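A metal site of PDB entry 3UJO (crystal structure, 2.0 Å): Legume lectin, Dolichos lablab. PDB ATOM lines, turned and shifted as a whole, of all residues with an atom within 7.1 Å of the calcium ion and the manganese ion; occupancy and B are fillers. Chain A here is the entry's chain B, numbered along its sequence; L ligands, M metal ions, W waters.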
ATOM      1  N   ASP A 108     -21.047  19.538  26.792  1.00  0.00           N
ATOM      2  CA  ASP A 108     -19.807  20.054  26.206  1.00  0.00           C
ATOM      3  C   ASP A 108     -19.232  21.260  26.955  1.00  0.00           C
ATOM      4  O   ASP A 108     -18.067  21.615  26.737  1.00  0.00           O
ATOM      5  CB  ASP A 108     -20.024  20.425  24.738  1.00  0.00           C
ATOM      6  CG  ASP A 108     -19.667  19.299  23.790  1.00  0.00           C
ATOM      7  OD1 ASP A 108     -18.476  18.918  23.737  1.00  0.00           O
ATOM      8  OD2 ASP A 108     -20.567  18.790  23.104  1.00  0.00           O
ATOM      9  N   GLY A 109     -20.033  21.873  27.817  1.00  0.00           N
ATOM     10  CA  GLY A 109     -19.616  23.046  28.593  1.00  0.00           C
ATOM     11  C   GLY A 109     -20.482  24.275  28.355  1.00  0.00           C
ATOM     12  O   GLY A 109     -21.429  24.228  27.572  1.00  0.00           O
ATOM     13  N   GLY A 125     -23.136  21.195  20.468  1.00  0.00           N
ATOM     14  CA  GLY A 125     -21.995  20.370  20.842  1.00  0.00           C
ATOM     15  C   GLY A 125     -20.728  21.122  21.157  1.00  0.00           C
ATOM     16  O   GLY A 125     -20.725  22.059  21.956  1.00  0.00           O
ATOM     17  N   GLY A 126     -19.623  20.705  20.528  1.00  0.00           N
ATOM     18  CA  GLY A 126     -18.310  21.306  20.747  1.00  0.00           C
ATOM     19  C   GLY A 126     -18.195  22.765  20.347  1.00  0.00           C
ATOM     20  O   GLY A 126     -17.240  23.438  20.719  1.00  0.00           O
ATOM     21  N   PHE A 127     -19.181  23.243  19.592  1.00  0.00           N
ATOM     22  CA  PHE A 127     -19.239  24.641  19.176  1.00  0.00           C
ATOM     23  C   PHE A 127     -19.975  25.504  20.196  1.00  0.00           C
ATOM     24  O   PHE A 127     -19.969  26.731  20.110  1.00  0.00           O
ATOM     25  CB  PHE A 127     -19.880  24.775  17.790  1.00  0.00           C
ATOM     26  CG  PHE A 127     -19.102  24.121  16.699  1.00  0.00           C
ATOM     27  CD1 PHE A 127     -18.055  24.795  16.070  1.00  0.00           C
ATOM     28  CD2 PHE A 127     -19.402  22.827  16.299  1.00  0.00           C
ATOM     29  CE1 PHE A 127     -17.327  24.182  15.053  1.00  0.00           C
ATOM     30  CE2 PHE A 127     -18.677  22.207  15.288  1.00  0.00           C
ATOM     31  CZ  PHE A 127     -17.638  22.888  14.662  1.00  0.00           C
ATOM     32  N   LEU A 128     -20.640  24.840  21.147  1.00  0.00           N
ATOM     33  CA  LEU A 128     -21.261  25.487  22.318  1.00  0.00           C
ATOM     34  C   LEU A 128     -22.403  26.461  22.006  1.00  0.00           C
ATOM     35  O   LEU A 128     -22.789  27.267  22.848  1.00  0.00           O
ATOM     36  CB  LEU A 128     -20.196  26.137  23.218  1.00  0.00           C
ATOM     37  CG  LEU A 128     -19.066  25.241  23.759  1.00  0.00           C
ATOM     38  CD1 LEU A 128     -17.921  26.074  24.320  1.00  0.00           C
ATOM     39  CD2 LEU A 128     -19.581  24.266  24.818  1.00  0.00           C
ATOM     40  N   GLU A 146     -15.061  30.557  27.174  1.00  0.00           N
ATOM     41  CA  GLU A 146     -15.616  29.218  27.298  1.00  0.00           C
ATOM     42  C   GLU A 146     -15.149  28.511  28.573  1.00  0.00           C
ATOM     43  O   GLU A 146     -14.042  28.730  29.066  1.00  0.00           O
ATOM     44  CB  GLU A 146     -15.319  28.368  26.056  1.00  0.00           C
ATOM     45  CG  GLU A 146     -13.842  28.053  25.827  1.00  0.00           C
ATOM     46  CD  GLU A 146     -13.626  26.946  24.808  1.00  0.00           C
ATOM     47  OE1 GLU A 146     -14.367  26.890  23.806  1.00  0.00           O
ATOM     48  OE2 GLU A 146     -12.690  26.146  25.001  1.00  0.00           O
ATOM     49  N   PHE A 147     -16.030  27.670  29.112  1.00  0.00           N
ATOM     50  CA  PHE A 147     -15.672  26.760  30.179  1.00  0.00           C
ATOM     51  C   PHE A 147     -15.945  25.353  29.643  1.00  0.00           C
ATOM     52  O   PHE A 147     -17.061  24.849  29.684  1.00  0.00           O
ATOM     53  CB  PHE A 147     -16.435  27.088  31.460  1.00  0.00           C
ATOM     54  CG  PHE A 147     -16.167  28.482  31.978  1.00  0.00           C
ATOM     55  CD1 PHE A 147     -15.046  28.740  32.759  1.00  0.00           C
ATOM     56  CD2 PHE A 147     -17.023  29.531  31.669  1.00  0.00           C
ATOM     57  CE1 PHE A 147     -14.784  30.031  33.228  1.00  0.00           C
ATOM     58  CE2 PHE A 147     -16.766  30.820  32.129  1.00  0.00           C
ATOM     59  CZ  PHE A 147     -15.649  31.071  32.917  1.00  0.00           C
ATOM     60  N   ASP A 148     -14.881  24.763  29.111  1.00  0.00           N
ATOM     61  CA  ASP A 148     -14.984  23.612  28.233  1.00  0.00           C
ATOM     62  C   ASP A 148     -14.651  22.320  28.977  1.00  0.00           C
ATOM     63  O   ASP A 148     -13.546  22.148  29.474  1.00  0.00           O
ATOM     64  CB  ASP A 148     -14.028  23.796  27.045  1.00  0.00           C
ATOM     65  CG  ASP A 148     -14.334  22.862  25.898  1.00  0.00           C
ATOM     66  OD1 ASP A 148     -14.845  21.742  26.130  1.00  0.00           O
ATOM     67  OD2 ASP A 148     -14.043  23.253  24.744  1.00  0.00           O
ATOM     68  N   THR A 149     -15.629  21.418  29.023  1.00  0.00           N
ATOM     69  CA  THR A 149     -15.475  20.133  29.704  1.00  0.00           C
ATOM     70  C   THR A 149     -15.470  18.928  28.751  1.00  0.00           C
ATOM     71  O   THR A 149     -15.809  17.812  29.153  1.00  0.00           O
ATOM     72  CB  THR A 149     -16.561  19.922  30.778  1.00  0.00           C
ATOM     73  OG1 THR A 149     -17.829  20.319  30.254  1.00  0.00           O
ATOM     74  CG2 THR A 149     -16.250  20.726  32.021  1.00  0.00           C
ATOM     75  N   PHE A 150     -15.101  19.157  27.494  1.00  0.00           N
ATOM     76  CA  PHE A 150     -14.950  18.069  26.530  1.00  0.00           C
ATOM     77  C   PHE A 150     -13.813  18.326  25.545  1.00  0.00           C
ATOM     78  O   PHE A 150     -13.789  19.342  24.856  1.00  0.00           O
ATOM     79  CB  PHE A 150     -16.259  17.790  25.781  1.00  0.00           C
ATOM     80  CG  PHE A 150     -16.187  16.615  24.845  1.00  0.00           C
ATOM     81  CD1 PHE A 150     -15.790  16.780  23.524  1.00  0.00           C
ATOM     82  CD2 PHE A 150     -16.506  15.329  25.295  1.00  0.00           C
ATOM     83  CE1 PHE A 150     -15.709  15.690  22.654  1.00  0.00           C
ATOM     84  CE2 PHE A 150     -16.437  14.240  24.433  1.00  0.00           C
ATOM     85  CZ  PHE A 150     -16.041  14.419  23.109  1.00  0.00           C
ATOM     86  N   TYR A 151     -12.890  17.371  25.491  1.00  0.00           N
ATOM     87  CA  TYR A 151     -11.754  17.412  24.587  1.00  0.00           C
ATOM     88  C   TYR A 151     -12.186  17.103  23.158  1.00  0.00           C
ATOM     89  O   TYR A 151     -12.421  15.941  22.803  1.00  0.00           O
ATOM     90  CB  TYR A 151     -10.682  16.421  25.077  1.00  0.00           C
ATOM     91  CG  TYR A 151      -9.403  16.353  24.263  1.00  0.00           C
ATOM     92  CD1 TYR A 151      -8.743  17.510  23.851  1.00  0.00           C
ATOM     93  CD2 TYR A 151      -8.827  15.128  23.946  1.00  0.00           C
ATOM     94  CE1 TYR A 151      -7.560  17.448  23.121  1.00  0.00           C
ATOM     95  CE2 TYR A 151      -7.642  15.053  23.219  1.00  0.00           C
ATOM     96  CZ  TYR A 151      -7.006  16.214  22.811  1.00  0.00           C
ATOM     97  OH  TYR A 151      -5.839  16.146  22.095  1.00  0.00           O
ATOM     98  N   ASN A 152     -12.295  18.151  22.335  1.00  0.00           N
ATOM     99  CA  ASN A 152     -12.683  17.989  20.935  1.00  0.00           C
ATOM    100  C   ASN A 152     -11.537  17.623  19.992  1.00  0.00           C
ATOM    101  O   ASN A 152     -11.755  17.044  18.934  1.00  0.00           O
ATOM    102  CB  ASN A 152     -13.414  19.243  20.428  1.00  0.00           C
ATOM    103  CG  ASN A 152     -14.907  19.220  20.757  1.00  0.00           C
ATOM    104  OD1 ASN A 152     -15.358  19.866  21.708  1.00  0.00           O
ATOM    105  ND2 ASN A 152     -15.677  18.469  19.973  1.00  0.00           N
ATOM    106  N   GLY A 153     -10.306  17.968  20.384  1.00  0.00           N
ATOM    107  CA  GLY A 153      -9.112  17.573  19.613  1.00  0.00           C
ATOM    108  C   GLY A 153      -8.875  18.389  18.366  1.00  0.00           C
ATOM    109  O   GLY A 153      -7.763  18.852  18.108  1.00  0.00           O
ATOM    110  N   TRP A 155      -9.397  21.214  17.923  1.00  0.00           N
ATOM    111  CA  TRP A 155      -8.959  22.531  18.353  1.00  0.00           C
ATOM    112  C   TRP A 155      -8.584  22.565  19.838  1.00  0.00           C
ATOM    113  O   TRP A 155      -7.732  23.357  20.244  1.00  0.00           O
ATOM    114  CB  TRP A 155     -10.041  23.575  18.048  1.00  0.00           C
ATOM    115  CG  TRP A 155     -11.428  23.235  18.547  1.00  0.00           C
ATOM    116  CD1 TRP A 155     -11.980  23.611  19.742  1.00  0.00           C
ATOM    117  CD2 TRP A 155     -12.437  22.474  17.869  1.00  0.00           C
ATOM    118  NE1 TRP A 155     -13.266  23.125  19.839  1.00  0.00           N
ATOM    119  CE2 TRP A 155     -13.571  22.431  18.706  1.00  0.00           C
ATOM    120  CE3 TRP A 155     -12.492  21.834  16.618  1.00  0.00           C
ATOM    121  CZ2 TRP A 155     -14.746  21.756  18.345  1.00  0.00           C
ATOM    122  CZ3 TRP A 155     -13.662  21.161  16.265  1.00  0.00           C
ATOM    123  CH2 TRP A 155     -14.773  21.133  17.119  1.00  0.00           C
ATOM    124  N   ASP A 156      -9.190  21.684  20.629  1.00  0.00           N
ATOM    125  CA  ASP A 156      -9.030  21.707  22.084  1.00  0.00           C
ATOM    126  C   ASP A 156      -7.666  21.254  22.622  1.00  0.00           C
ATOM    127  O   ASP A 156      -7.029  20.369  22.039  1.00  0.00           O
ATOM    128  CB  ASP A 156     -10.128  20.881  22.757  1.00  0.00           C
ATOM    129  CG  ASP A 156     -11.424  21.662  22.935  1.00  0.00           C
ATOM    130  OD1 ASP A 156     -11.370  22.914  22.948  1.00  0.00           O
ATOM    131  OD2 ASP A 156     -12.487  21.026  23.090  1.00  0.00           O
ATOM    132  N   PRO A 157      -7.217  21.867  23.728  1.00  0.00           N
ATOM    133  CA  PRO A 157      -6.134  21.316  24.542  1.00  0.00           C
ATOM    134  C   PRO A 157      -6.612  20.059  25.286  1.00  0.00           C
ATOM    135  O   PRO A 157      -7.820  19.835  25.382  1.00  0.00           O
ATOM    136  CB  PRO A 157      -5.822  22.436  25.548  1.00  0.00           C
ATOM    137  CG  PRO A 157      -6.386  23.674  24.934  1.00  0.00           C
ATOM    138  CD  PRO A 157      -7.589  23.225  24.181  1.00  0.00           C
ATOM    139  N   HIS A 161     -10.788  22.978  30.305  1.00  0.00           N
ATOM    140  CA  HIS A 161     -10.131  24.265  30.084  1.00  0.00           C
ATOM    141  C   HIS A 161     -11.053  25.470  29.962  1.00  0.00           C
ATOM    142  O   HIS A 161     -12.211  25.355  29.562  1.00  0.00           O
ATOM    143  CB  HIS A 161      -9.227  24.185  28.851  1.00  0.00           C
ATOM    144  CG  HIS A 161      -9.938  23.836  27.582  1.00  0.00           C
ATOM    145  ND1 HIS A 161     -10.228  22.533  27.231  1.00  0.00           N
ATOM    146  CD2 HIS A 161     -10.413  24.611  26.577  1.00  0.00           C
ATOM    147  CE1 HIS A 161     -10.855  22.528  26.070  1.00  0.00           C
ATOM    148  NE2 HIS A 161     -10.979  23.776  25.656  1.00  0.00           N
ATOM    149  N   ILE A 162     -10.510  26.615  30.352  1.00  0.00           N
ATOM    150  CA  ILE A 162     -11.107  27.914  30.081  1.00  0.00           C
ATOM    151  C   ILE A 162     -10.404  28.459  28.844  1.00  0.00           C
ATOM    152  O   ILE A 162      -9.179  28.348  28.729  1.00  0.00           O
ATOM    153  CB  ILE A 162     -10.939  28.884  31.279  1.00  0.00           C
ATOM    154  CG1 ILE A 162     -11.389  28.227  32.588  1.00  0.00           C
ATOM    155  CG2 ILE A 162     -11.716  30.185  31.039  1.00  0.00           C
ATOM    156  CD1 ILE A 162     -10.998  28.974  33.846  1.00  0.00           C
ATOM    157  N   GLY A 163     -11.176  29.007  27.913  1.00  0.00           N
ATOM    158  CA  GLY A 163     -10.614  29.560  26.676  1.00  0.00           C
ATOM    159  C   GLY A 163     -11.189  30.913  26.315  1.00  0.00           C
ATOM    160  O   GLY A 163     -12.324  31.245  26.659  1.00  0.00           O
ATOM    161  N   ASP A 165     -12.382  32.949  23.127  1.00  0.00           N
ATOM    162  CA  ASP A 165     -12.831  32.655  21.770  1.00  0.00           C
ATOM    163  C   ASP A 165     -13.133  33.920  20.986  1.00  0.00           C
ATOM    164  O   ASP A 165     -14.037  34.683  21.346  1.00  0.00           O
ATOM    165  CB  ASP A 165     -14.072  31.750  21.793  1.00  0.00           C
ATOM    166  CG  ASP A 165     -13.788  30.380  22.381  1.00  0.00           C
ATOM    167  OD1 ASP A 165     -12.679  30.164  22.932  1.00  0.00           O
ATOM    168  OD2 ASP A 165     -14.676  29.506  22.309  1.00  0.00           O
ATOM    169  N   ILE A 169     -14.134  28.746  17.414  1.00  0.00           N
ATOM    170  CA  ILE A 169     -14.172  27.804  18.544  1.00  0.00           C
ATOM    171  C   ILE A 169     -12.760  27.319  18.899  1.00  0.00           C
ATOM    172  O   ILE A 169     -12.513  26.782  19.989  1.00  0.00           O
ATOM    173  CB  ILE A 169     -15.159  26.620  18.271  1.00  0.00           C
ATOM    174  CG1 ILE A 169     -15.444  25.818  19.548  1.00  0.00           C
ATOM    175  CG2 ILE A 169     -14.645  25.713  17.134  1.00  0.00           C
ATOM    176  CD1 ILE A 169     -16.246  26.581  20.591  1.00  0.00           C
ATOM    177  N   LYS A 170     -11.830  27.529  17.971  1.00  0.00           N
ATOM    178  CA  LYS A 170     -10.398  27.359  18.219  1.00  0.00           C
ATOM    179  C   LYS A 170      -9.918  28.551  19.031  1.00  0.00           C
ATOM    180  O   LYS A 170      -9.739  29.646  18.497  1.00  0.00           O
ATOM    181  CB  LYS A 170      -9.653  27.260  16.892  1.00  0.00           C
ATOM    182  CG  LYS A 170      -8.233  26.710  16.964  1.00  0.00           C
ATOM    183  CD  LYS A 170      -7.825  26.148  15.621  1.00  0.00           C
ATOM    184  CE  LYS A 170      -6.360  25.739  15.581  1.00  0.00           C
ATOM    185  NZ  LYS A 170      -6.054  24.986  14.334  1.00  0.00           N
ATOM    186  N   SER A 171      -9.701  28.328  20.327  1.00  0.00           N
ATOM    187  CA  SER A 171      -9.353  29.387  21.276  1.00  0.00           C
ATOM    188  C   SER A 171      -8.003  30.052  20.972  1.00  0.00           C
ATOM    189  O   SER A 171      -7.037  29.382  20.595  1.00  0.00           O
ATOM    190  CB  SER A 171      -9.359  28.855  22.713  1.00  0.00           C
ATOM    191  OG  SER A 171     -10.618  28.305  23.063  1.00  0.00           O
ATOM    192  N   THR A 174      -5.713  29.519  26.091  1.00  0.00           N
ATOM    193  CA  THR A 174      -6.365  28.591  27.013  1.00  0.00           C
ATOM    194  C   THR A 174      -5.589  28.502  28.319  1.00  0.00           C
ATOM    195  O   THR A 174      -4.418  28.874  28.392  1.00  0.00           O
ATOM    196  CB  THR A 174      -6.499  27.173  26.404  1.00  0.00           C
ATOM    197  OG1 THR A 174      -5.247  26.801  25.804  1.00  0.00           O
ATOM    198  CG2 THR A 174      -7.588  27.129  25.347  1.00  0.00           C
HETATM  199  C1  LIG L   1     -19.270  14.792  19.234  1.00  0.00           C
HETATM  200  C2  LIG L   1     -19.161  16.309  19.380  1.00  0.00           C
HETATM  201  C3  LIG L   1     -18.602  16.657  20.764  1.00  0.00           C
HETATM  202  C4  LIG L   1     -19.413  15.960  21.851  1.00  0.00           C
HETATM  203  C5  LIG L   1     -19.448  14.455  21.592  1.00  0.00           C
HETATM  204  C6  LIG L   1     -20.279  13.724  22.642  1.00  0.00           C
HETATM  205  O1  LIG L   1     -19.981  14.511  18.057  1.00  0.00           O
HETATM  206  O2  LIG L   1     -18.342  16.857  18.369  1.00  0.00           O
HETATM  207  O3  LIG L   1     -18.623  18.042  20.966  1.00  0.00           O
HETATM  208  O4  LIG L   1     -20.732  16.483  21.844  1.00  0.00           O
HETATM  209  O5  LIG L   1     -19.989  14.218  20.309  1.00  0.00           O
HETATM  210  O6  LIG L   1     -19.913  12.372  22.676  1.00  0.00           O
HETATM  211 CA    CA M   1     -14.878  21.230  23.530  1.00  0.00          CA
HETATM  212 MN    MN M   2     -12.200  24.510  23.830  1.00  0.00          MN
HETATM  213  O   HOH W   1     -15.100  22.883  21.911  1.00  0.00           O
HETATM  214  O   HOH W   2     -13.181  25.201  22.375  1.00  0.00           O
HETATM  215  O   HOH W   3     -10.332  25.659  23.369  1.00  0.00           O
HETATM  216  O   HOH W   4     -16.825  20.903  24.449  1.00  0.00           O
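Water W1 lies within hydrogen-bond range of O of Gly 126 (2.5 Å) and NE1 of Trp 155 (2.8 Å).
Water W2 lies within hydrogen-bond range of the side-chain carboxylate (OE1) of Glu 146, the backbone carbonyl oxygen (O) of Ile 169 and the indole nitrogen (NE1) of Trp 155.
Four residues have an atom within 4 Å of the manganese ion: Glu 146, Asp 148, Asp 156 and His 161.
Along chain A the residues within 4 Å of the manganese ion span positions 146 to 161.
The nearest printed residue that does not touch the manganese ion is Ser 171 (4.2 Å).
Within 4 Å of the calcium ion: Asp 148, Phe 150, Asn 152 and Asp 156.
Along chain A the residues within 4 Å of the calcium ion span positions 148 to 156.
The nearest printed residue that does not touch the calcium ion is Asp 108 (4.3 Å).
The side-chain amide nitrogen (ND2) of Asn 152 lies within hydrogen-bond range of an oxygen (O3) of the ligand (3.1 Å).
The side-chain carboxylate of Asp 108 sits at hydrogen-bond distance from an oxygen (O4) of the ligand (2.6 Å).
The backbone NH of Gly 126 is in hydrogen-bond range of an oxygen (O3) of the ligand (2.9 Å).
The backbone NH of Glu 146 lies within hydrogen-bond range of the backbone carbonyl oxygen of Gly 163 (2.9 Å).
The manganese ion is bound by water W2, OD1 of Asp 156, OE2 of Glu 146, water W3, NE2 of His 161 and OD2 of Asp 148.
Water W4 binds the calcium ion, at 2.2 Å.
Water W1 is bound to the calcium ion, 2.3 Å away.
The side-chain amide oxygen (OD1) of Asn 152 binds the calcium ion (2.3 Å).
OD2 of Asp 156 is bound to the calcium ion, 2.4 Å away.
The calcium ion is bound by OD2 of Asp 148 (2.5 Å).
O of Phe 150 is bound to the calcium ion (2.6 Å).
OD1 of Asp 148 binds the calcium ion (2.7 Å).
The calcium ion has seven donor atoms within binding distance.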
